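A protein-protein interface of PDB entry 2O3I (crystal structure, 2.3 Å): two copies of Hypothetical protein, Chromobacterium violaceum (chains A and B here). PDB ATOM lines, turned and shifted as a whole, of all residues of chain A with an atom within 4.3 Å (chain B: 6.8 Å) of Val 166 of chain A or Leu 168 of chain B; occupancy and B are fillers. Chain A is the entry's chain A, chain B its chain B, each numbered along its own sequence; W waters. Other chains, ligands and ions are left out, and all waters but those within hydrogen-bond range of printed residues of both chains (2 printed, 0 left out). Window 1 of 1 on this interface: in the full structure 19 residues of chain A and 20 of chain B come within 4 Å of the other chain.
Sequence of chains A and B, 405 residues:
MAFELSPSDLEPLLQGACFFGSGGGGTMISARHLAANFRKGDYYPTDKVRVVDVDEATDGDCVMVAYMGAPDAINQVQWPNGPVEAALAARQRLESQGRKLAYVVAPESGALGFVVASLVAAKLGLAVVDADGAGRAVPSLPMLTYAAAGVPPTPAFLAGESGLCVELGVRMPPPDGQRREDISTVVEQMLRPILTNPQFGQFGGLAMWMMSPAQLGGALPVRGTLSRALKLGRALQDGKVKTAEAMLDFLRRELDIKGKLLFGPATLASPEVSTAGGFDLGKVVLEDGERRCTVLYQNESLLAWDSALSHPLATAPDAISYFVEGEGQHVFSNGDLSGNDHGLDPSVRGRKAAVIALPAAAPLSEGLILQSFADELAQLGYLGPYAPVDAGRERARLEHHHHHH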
ATOM      1  N   ALA A 156       2.626  21.362  23.642  1.00  0.00           N
ATOM      2  CA  ALA A 156       1.863  22.586  23.859  1.00  0.00           C
ATOM      3  C   ALA A 156       0.957  22.723  22.632  1.00  0.00           C
ATOM      4  O   ALA A 156       1.379  22.439  21.510  1.00  0.00           O
ATOM      5  CB  ALA A 156       2.791  23.778  23.967  1.00  0.00           C
ATOM      6  N   PHE A 157      -0.285  23.143  22.837  1.00  0.00           N
ATOM      7  CA  PHE A 157      -1.196  23.274  21.713  1.00  0.00           C
ATOM      8  C   PHE A 157      -1.709  24.703  21.552  1.00  0.00           C
ATOM      9  O   PHE A 157      -2.228  25.291  22.495  1.00  0.00           O
ATOM     10  CB  PHE A 157      -2.386  22.318  21.889  1.00  0.00           C
ATOM     11  CG  PHE A 157      -1.994  20.866  22.052  1.00  0.00           C
ATOM     12  CD1 PHE A 157      -1.551  20.116  20.959  1.00  0.00           C
ATOM     13  CD2 PHE A 157      -2.046  20.258  23.300  1.00  0.00           C
ATOM     14  CE1 PHE A 157      -1.162  18.772  21.112  1.00  0.00           C
ATOM     15  CE2 PHE A 157      -1.662  18.922  23.467  1.00  0.00           C
ATOM     16  CZ  PHE A 157      -1.218  18.177  22.369  1.00  0.00           C
ATOM     17  N   LEU A 158      -1.531  25.259  20.355  1.00  0.00           N
ATOM     18  CA  LEU A 158      -2.014  26.596  20.026  1.00  0.00           C
ATOM     19  C   LEU A 158      -3.105  26.401  18.977  1.00  0.00           C
ATOM     20  O   LEU A 158      -2.924  25.650  18.020  1.00  0.00           O
ATOM     21  CB  LEU A 158      -0.895  27.462  19.454  1.00  0.00           C
ATOM     22  CG  LEU A 158       0.157  27.952  20.441  1.00  0.00           C
ATOM     23  CD1 LEU A 158       1.274  28.637  19.657  1.00  0.00           C
ATOM     24  CD2 LEU A 158      -0.467  28.903  21.456  1.00  0.00           C
ATOM     25  N   LEU A 164      -7.637  25.808  12.815  1.00  0.00           N
ATOM     26  CA  LEU A 164      -6.185  25.725  12.772  1.00  0.00           C
ATOM     27  C   LEU A 164      -5.644  25.329  14.154  1.00  0.00           C
ATOM     28  O   LEU A 164      -6.008  25.923  15.167  1.00  0.00           O
ATOM     29  CB  LEU A 164      -5.627  27.080  12.312  1.00  0.00           C
ATOM     30  CG  LEU A 164      -4.140  27.463  12.308  1.00  0.00           C
ATOM     31  CD1 LEU A 164      -3.752  27.933  13.678  1.00  0.00           C
ATOM     32  CD2 LEU A 164      -3.276  26.310  11.847  1.00  0.00           C
ATOM     33  N   CYS A 165      -4.806  24.294  14.186  1.00  0.00           N
ATOM     34  CA  CYS A 165      -4.200  23.803  15.422  1.00  0.00           C
ATOM     35  C   CYS A 165      -2.717  23.542  15.191  1.00  0.00           C
ATOM     36  O   CYS A 165      -2.333  22.909  14.208  1.00  0.00           O
ATOM     37  CB  CYS A 165      -4.875  22.507  15.893  1.00  0.00           C
ATOM     38  SG  CYS A 165      -4.051  21.695  17.308  1.00  0.00           S
ATOM     39  N   VAL A 166      -1.888  24.040  16.098  1.00  0.00           N
ATOM     40  CA  VAL A 166      -0.449  23.867  16.004  1.00  0.00           C
ATOM     41  C   VAL A 166       0.066  23.231  17.291  1.00  0.00           C
ATOM     42  O   VAL A 166      -0.340  23.618  18.391  1.00  0.00           O
ATOM     43  CB  VAL A 166       0.275  25.227  15.796  1.00  0.00           C
ATOM     44  CG1 VAL A 166       1.775  25.017  15.723  1.00  0.00           C
ATOM     45  CG2 VAL A 166      -0.213  25.890  14.522  1.00  0.00           C
ATOM     46  N   GLU A 167       0.949  22.248  17.150  1.00  0.00           N
ATOM     47  CA  GLU A 167       1.527  21.589  18.311  1.00  0.00           C
ATOM     48  C   GLU A 167       3.012  21.924  18.393  1.00  0.00           C
ATOM     49  O   GLU A 167       3.704  22.014  17.373  1.00  0.00           O
ATOM     50  CB  GLU A 167       1.348  20.080  18.220  1.00  0.00           C
ATOM     51  CG  GLU A 167       1.878  19.343  19.434  1.00  0.00           C
ATOM     52  CD  GLU A 167       1.812  17.835  19.284  1.00  0.00           C
ATOM     53  OE1 GLU A 167       0.792  17.323  18.771  1.00  0.00           O
ATOM     54  OE2 GLU A 167       2.775  17.162  19.689  1.00  0.00           O
ATOM     55  N   LEU A 168       3.504  22.104  19.609  1.00  0.00           N
ATOM     56  CA  LEU A 168       4.904  22.428  19.796  1.00  0.00           C
ATOM     57  C   LEU A 168       5.521  21.560  20.886  1.00  0.00           C
ATOM     58  O   LEU A 168       4.984  21.454  21.985  1.00  0.00           O
ATOM     59  CB  LEU A 168       5.040  23.912  20.146  1.00  0.00           C
ATOM     60  CG  LEU A 168       6.394  24.626  20.067  1.00  0.00           C
ATOM     61  CD1 LEU A 168       7.238  24.266  21.252  1.00  0.00           C
ATOM     62  CD2 LEU A 168       7.097  24.288  18.763  1.00  0.00           C
ATOM     63  N   PHE A 200      -3.171  32.825  12.553  1.00  0.00           N
ATOM     64  CA  PHE A 200      -3.656  33.025  13.917  1.00  0.00           C
ATOM     65  C   PHE A 200      -4.310  34.392  14.104  1.00  0.00           C
ATOM     66  O   PHE A 200      -5.400  34.493  14.664  1.00  0.00           O
ATOM     67  CB  PHE A 200      -2.515  32.875  14.929  1.00  0.00           C
ATOM     68  CG  PHE A 200      -2.267  31.464  15.358  1.00  0.00           C
ATOM     69  CD1 PHE A 200      -1.194  30.744  14.845  1.00  0.00           C
ATOM     70  CD2 PHE A 200      -3.114  30.848  16.278  1.00  0.00           C
ATOM     71  CE1 PHE A 200      -0.965  29.430  15.240  1.00  0.00           C
ATOM     72  CE2 PHE A 200      -2.894  29.533  16.680  1.00  0.00           C
ATOM     73  CZ  PHE A 200      -1.819  28.821  16.162  1.00  0.00           C
ATOM     74  N   PRO B 153       3.458  17.772   5.808  1.00  0.00           N
ATOM     75  CA  PRO B 153       4.741  18.339   6.238  1.00  0.00           C
ATOM     76  C   PRO B 153       5.166  18.029   7.676  1.00  0.00           C
ATOM     77  O   PRO B 153       6.347  17.826   7.955  1.00  0.00           O
ATOM     78  CB  PRO B 153       4.540  19.839   6.017  1.00  0.00           C
ATOM     79  CG  PRO B 153       3.085  20.013   6.377  1.00  0.00           C
ATOM     80  CD  PRO B 153       2.444  18.834   5.651  1.00  0.00           C
ATOM     81  N   THR B 154       4.209  18.005   8.591  1.00  0.00           N
ATOM     82  CA  THR B 154       4.536  17.742   9.984  1.00  0.00           C
ATOM     83  C   THR B 154       4.010  16.380  10.405  1.00  0.00           C
ATOM     84  O   THR B 154       3.135  15.825   9.752  1.00  0.00           O
ATOM     85  CB  THR B 154       3.946  18.836  10.899  1.00  0.00           C
ATOM     86  OG1 THR B 154       2.521  18.744  10.899  1.00  0.00           O
ATOM     87  CG2 THR B 154       4.343  20.218  10.392  1.00  0.00           C
ATOM     88  N   PRO B 155       4.531  15.824  11.509  1.00  0.00           N
ATOM     89  CA  PRO B 155       5.568  16.368  12.395  1.00  0.00           C
ATOM     90  C   PRO B 155       6.876  16.760  11.706  1.00  0.00           C
ATOM     91  O   PRO B 155       7.438  16.007  10.905  1.00  0.00           O
ATOM     92  CB  PRO B 155       5.782  15.244  13.411  1.00  0.00           C
ATOM     93  CG  PRO B 155       4.442  14.577  13.476  1.00  0.00           C
ATOM     94  CD  PRO B 155       4.042  14.526  12.017  1.00  0.00           C
ATOM     95  N   ALA B 156       7.346  17.958  12.028  1.00  0.00           N
ATOM     96  CA  ALA B 156       8.596  18.465  11.502  1.00  0.00           C
ATOM     97  C   ALA B 156       9.504  18.604  12.726  1.00  0.00           C
ATOM     98  O   ALA B 156       9.045  18.999  13.801  1.00  0.00           O
ATOM     99  CB  ALA B 156       8.375  19.820  10.835  1.00  0.00           C
ATOM    100  N   PHE B 157      10.782  18.275  12.567  1.00  0.00           N
ATOM    101  CA  PHE B 157      11.732  18.346  13.676  1.00  0.00           C
ATOM    102  C   PHE B 157      12.922  19.257  13.400  1.00  0.00           C
ATOM    103  O   PHE B 157      13.632  19.081  12.412  1.00  0.00           O
ATOM    104  CB  PHE B 157      12.264  16.950  13.991  1.00  0.00           C
ATOM    105  CG  PHE B 157      11.195  15.935  14.244  1.00  0.00           C
ATOM    106  CD1 PHE B 157      10.555  15.871  15.479  1.00  0.00           C
ATOM    107  CD2 PHE B 157      10.841  15.024  13.255  1.00  0.00           C
ATOM    108  CE1 PHE B 157       9.576  14.904  15.723  1.00  0.00           C
ATOM    109  CE2 PHE B 157       9.870  14.059  13.489  1.00  0.00           C
ATOM    110  CZ  PHE B 157       9.235  13.997  14.726  1.00  0.00           C
ATOM    111  N   LEU B 158      13.130  20.230  14.279  1.00  0.00           N
ATOM    112  CA  LEU B 158      14.253  21.151  14.169  1.00  0.00           C
ATOM    113  C   LEU B 158      15.190  20.828  15.327  1.00  0.00           C
ATOM    114  O   LEU B 158      14.757  20.744  16.472  1.00  0.00           O
ATOM    115  CB  LEU B 158      13.784  22.609  14.273  1.00  0.00           C
ATOM    116  CG  LEU B 158      13.111  23.260  13.058  1.00  0.00           C
ATOM    117  CD1 LEU B 158      12.690  24.683  13.414  1.00  0.00           C
ATOM    118  CD2 LEU B 158      14.067  23.285  11.867  1.00  0.00           C
ATOM    119  N   VAL B 166      13.208  20.592  18.713  1.00  0.00           N
ATOM    120  CA  VAL B 166      11.863  21.148  18.703  1.00  0.00           C
ATOM    121  C   VAL B 166      10.989  20.414  17.685  1.00  0.00           C
ATOM    122  O   VAL B 166      11.459  20.014  16.613  1.00  0.00           O
ATOM    123  CB  VAL B 166      11.900  22.652  18.341  1.00  0.00           C
ATOM    124  CG1 VAL B 166      10.493  23.230  18.322  1.00  0.00           C
ATOM    125  CG2 VAL B 166      12.772  23.397  19.330  1.00  0.00           C
ATOM    126  N   GLU B 167       9.718  20.231  18.027  1.00  0.00           N
ATOM    127  CA  GLU B 167       8.799  19.568  17.129  1.00  0.00           C
ATOM    128  C   GLU B 167       7.662  20.509  16.786  1.00  0.00           C
ATOM    129  O   GLU B 167       7.160  21.230  17.643  1.00  0.00           O
ATOM    130  CB  GLU B 167       8.230  18.302  17.768  1.00  0.00           C
ATOM    131  CG  GLU B 167       7.465  17.423  16.790  1.00  0.00           C
ATOM    132  CD  GLU B 167       6.646  16.358  17.490  1.00  0.00           C
ATOM    133  OE1 GLU B 167       7.066  15.902  18.571  1.00  0.00           O
ATOM    134  OE2 GLU B 167       5.587  15.966  16.956  1.00  0.00           O
ATOM    135  N   LEU B 168       7.269  20.510  15.522  1.00  0.00           N
ATOM    136  CA  LEU B 168       6.175  21.353  15.076  1.00  0.00           C
ATOM    137  C   LEU B 168       5.148  20.502  14.346  1.00  0.00           C
ATOM    138  O   LEU B 168       5.492  19.657  13.510  1.00  0.00           O
ATOM    139  CB  LEU B 168       6.679  22.457  14.142  1.00  0.00           C
ATOM    140  CG  LEU B 168       5.662  23.522  13.722  1.00  0.00           C
ATOM    141  CD1 LEU B 168       5.258  24.357  14.933  1.00  0.00           C
ATOM    142  CD2 LEU B 168       6.273  24.425  12.659  1.00  0.00           C
ATOM    143  N   GLY B 169       3.885  20.717  14.697  1.00  0.00           N
ATOM    144  CA  GLY B 169       2.793  19.999  14.073  1.00  0.00           C
ATOM    145  C   GLY B 169       1.831  21.066  13.595  1.00  0.00           C
ATOM    146  O   GLY B 169       1.632  22.072  14.283  1.00  0.00           O
ATOM    147  N   VAL B 170       1.250  20.877  12.414  1.00  0.00           N
ATOM    148  CA  VAL B 170       0.304  21.846  11.884  1.00  0.00           C
ATOM    149  C   VAL B 170      -0.887  21.157  11.237  1.00  0.00           C
ATOM    150  O   VAL B 170      -0.732  20.306  10.360  1.00  0.00           O
ATOM    151  CB  VAL B 170       0.958  22.770  10.838  1.00  0.00           C
ATOM    152  CG1 VAL B 170      -0.074  23.748  10.299  1.00  0.00           C
ATOM    153  CG2 VAL B 170       2.128  23.520  11.459  1.00  0.00           C
ATOM    154  N   ARG B 171      -2.076  21.526  11.694  1.00  0.00           N
ATOM    155  CA  ARG B 171      -3.323  20.987  11.164  1.00  0.00           C
ATOM    156  C   ARG B 171      -4.173  22.214  10.860  1.00  0.00           C
ATOM    157  O   ARG B 171      -4.525  22.967  11.764  1.00  0.00           O
ATOM    158  CB  ARG B 171      -4.014  20.102  12.205  1.00  0.00           C
ATOM    159  N   VAL B 186       2.773  27.878   5.233  1.00  0.00           N
ATOM    160  CA  VAL B 186       2.481  28.175   6.626  1.00  0.00           C
ATOM    161  C   VAL B 186       3.544  27.543   7.524  1.00  0.00           C
ATOM    162  O   VAL B 186       4.031  28.177   8.464  1.00  0.00           O
ATOM    163  CB  VAL B 186       1.080  27.637   7.031  1.00  0.00           C
ATOM    164  CG1 VAL B 186       0.829  27.877   8.514  1.00  0.00           C
ATOM    165  CG2 VAL B 186       0.003  28.329   6.209  1.00  0.00           C
ATOM    166  N   VAL B 187       3.901  26.298   7.222  1.00  0.00           N
ATOM    167  CA  VAL B 187       4.895  25.569   8.000  1.00  0.00           C
ATOM    168  C   VAL B 187       6.250  26.246   7.936  1.00  0.00           C
ATOM    169  O   VAL B 187       6.933  26.374   8.947  1.00  0.00           O
ATOM    170  CB  VAL B 187       5.026  24.103   7.504  1.00  0.00           C
ATOM    171  CG1 VAL B 187       6.291  23.455   8.069  1.00  0.00           C
ATOM    172  CG2 VAL B 187       3.796  23.307   7.928  1.00  0.00           C
ATOM    173  N   GLU B 188       6.633  26.692   6.743  1.00  0.00           N
ATOM    174  CA  GLU B 188       7.920  27.349   6.575  1.00  0.00           C
ATOM    175  C   GLU B 188       7.964  28.678   7.322  1.00  0.00           C
ATOM    176  O   GLU B 188       9.002  29.052   7.880  1.00  0.00           O
ATOM    177  CB  GLU B 188       8.216  27.588   5.094  1.00  0.00           C
ATOM    178  CG  GLU B 188       9.635  28.067   4.849  1.00  0.00           C
ATOM    179  CD  GLU B 188       9.907  28.387   3.399  1.00  0.00           C
ATOM    180  OE1 GLU B 188       9.373  29.398   2.908  1.00  0.00           O
ATOM    181  OE2 GLU B 188      10.653  27.628   2.750  1.00  0.00           O
ATOM    182  N   MET B 190       6.647  29.321  10.009  1.00  0.00           N
ATOM    183  CA  MET B 190       6.730  29.081  11.441  1.00  0.00           C
ATOM    184  C   MET B 190       8.076  28.462  11.792  1.00  0.00           C
ATOM    185  O   MET B 190       8.660  28.775  12.832  1.00  0.00           O
ATOM    186  CB  MET B 190       5.594  28.169  11.896  1.00  0.00           C
ATOM    187  CG  MET B 190       4.209  28.768  11.720  1.00  0.00           C
ATOM    188  SD  MET B 190       2.805  27.608  12.388  1.00  0.00           S
ATOM    189  CE  MET B 190       1.403  28.911  12.607  1.00  0.00           C
ATOM    190  N   LEU B 191       8.569  27.592  10.913  1.00  0.00           N
ATOM    191  CA  LEU B 191       9.855  26.932  11.127  1.00  0.00           C
ATOM    192  C   LEU B 191      11.018  27.917  11.215  1.00  0.00           C
ATOM    193  O   LEU B 191      11.865  27.814  12.104  1.00  0.00           O
ATOM    194  CB  LEU B 191      10.150  25.938   9.997  1.00  0.00           C
ATOM    195  CG  LEU B 191       9.368  24.626   9.920  1.00  0.00           C
ATOM    196  CD1 LEU B 191       9.912  23.779   8.771  1.00  0.00           C
ATOM    197  CD2 LEU B 191       9.496  23.874  11.230  1.00  0.00           C
ATOM    198  N   ILE B 194      11.483  30.149  14.429  1.00  0.00           N
ATOM    199  CA  ILE B 194      11.931  29.324  15.545  1.00  0.00           C
ATOM    200  C   ILE B 194      13.447  29.231  15.565  1.00  0.00           C
ATOM    201  O   ILE B 194      14.062  29.225  16.627  1.00  0.00           O
ATOM    202  CB  ILE B 194      11.332  27.905  15.466  1.00  0.00           C
ATOM    203  CG1 ILE B 194       9.819  27.987  15.660  1.00  0.00           C
ATOM    204  CG2 ILE B 194      11.969  26.997  16.516  1.00  0.00           C
ATOM    205  CD1 ILE B 194       9.104  26.656  15.540  1.00  0.00           C
HETATM  206  O   HOH W   1       3.824  14.949  18.839  1.00  0.00           O
HETATM  207  O   HOH W   2       5.161  18.014  20.416  1.00  0.00           O
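The backbone NH (N) of Glu 167 of chain A sits at hydrogen-bond distance from the backbone carbonyl oxygen (O) of Gly 169 of chain B (3.0 Å).
The backbone NH (N) of Cys 165 of chain A sits at hydrogen-bond distance from the backbone carbonyl oxygen (O) of Arg 171 of chain B, at 2.8 Å.
The side-chain hydroxyl of Thr 154 of chain B sits at hydrogen-bond distance from the backbone NH of Val 170 of chain B, at 2.9 Å.
The backbone NH (N) of Val 166 of chain A is in hydrogen-bond range of the backbone carbonyl oxygen (O) of Leu 158 of chain A (2.7 Å).
The backbone carbonyl oxygen (O) of Ala 156 of chain B sits at hydrogen-bond distance from the backbone NH (N) of Leu 168 of chain B (2.9 Å).
N of Val 166 of chain B is in hydrogen-bond range of O of Leu 158 of chain B, 2.7 Å away.
N of Leu 168 of chain A sits at hydrogen-bond distance from O of Ala 156 of chain A (2.9 Å).
O of Arg 171 of chain B touches CA of Leu 164 of chain A, at 3.4 Å.
Val 170 of chain B touches Cys 165 of chain A.
Val 166 of chain A touches Leu 168 of chain B (CG1 to CD1, 3.6 Å).
O of Gly 169 of chain B touches CA of Val 166 of chain A, at 3.2 Å.
Val 166 of chain A touches Met 190 of chain B (CG2 to CE, 3.9 Å).
O of Glu 167 of chain A touches O of Glu 167 of chain B, at 3.6 Å.
Glu 167 of chain A touches Leu 168 of chain B (O to CA, 3.4 Å).
Val 166 of chain B touches Leu 168 of chain A (CG1 to CD2, 3.6 Å).
CD2 of Leu 168 of chain A touches O of Glu 167 of chain B, at 3.3 Å.
Phe 200 of chain A touches Met 190 of chain B (CE1 to CE, 3.6 Å).
Leu 158 of chain A touches none of the printed residues of chain B.
Of the printed residues of chain B, Cys 165 of chain A touches Val 170 (3.7 Å) and Arg 171 (2.8 Å).
Of chain B, only Leu 168 (3.6 Å), Gly 169 (3.2 Å) and Met 190 (3.9 Å) come within 4 Å of Val 166 of chain A.
Printed residues of chain A within 4 Å of Val 166 of chain B: Leu 168 (3.6 Å).
Of the printed residues of chain A, Glu 167 of chain B touches Glu 167 (3.6 Å) and Leu 168 (3.3 Å).
Leu 168 of chain B touches just these residues of chain A: Val 166 (3.6 Å) and Glu 167 (3.4 Å).
Of the printed residues of chain A, Arg 171 of chain B touches Leu 164 (3.4 Å) and Cys 165 (2.8 Å).
The nearest residue of chain B that does not touch Val 166 of chain A is Val 170 of chain B (4.5 Å).
The nearest residue of chain A that does not touch Leu 168 of chain B is Leu 168 of chain A (4.2 Å).
The nearest printed residue of chain B that does not touch Leu 164 of chain A is Val 170 of chain B (4.4 Å).
Of the 18 printed residues of chain B, 7 touch a printed residue of chain A.
Hydrophobic or aromatic side chains of chain B that line the printed part of chain A: Val 166, Leu 168 and Met 190.
Hydrophobic or aromatic side chains of chain A within 4 Å of the printed part of chain B: Leu 164, Val 166, Leu 168 and Phe 200.
Among the printed residues, 12 pairs touch across the chains.
Val 166 of chain A touches Leu 168 of chain B, and with the chains exchanged Leu 168 of chain A touches Val 166 of chain B.
Glu 167 of chain A touches its own counterpart, Glu 167 of chain B.
Glu 167 of chain A touches Leu 168 of chain B, and with the chains exchanged Leu 168 of chain A touches Glu 167 of chain B.
6 positions are printed for both chains.
Of the 12 pairs that touch across the chains among the printed residues, 5 have their exchanged pair printed and touching as well.
Water W1 lies within hydrogen-bond range of the side-chain carboxylate (OE2) of Glu 167 of chain A (2.6 Å) and the side-chain carboxylate (OE2) of Glu 167 of chain B (2.8 Å).
Water W2 bridges the side-chain carboxylate of Glu 167 of chain A (2.6 Å) and the side-chain carboxylate of Glu 167 of chain B (3.4 Å).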
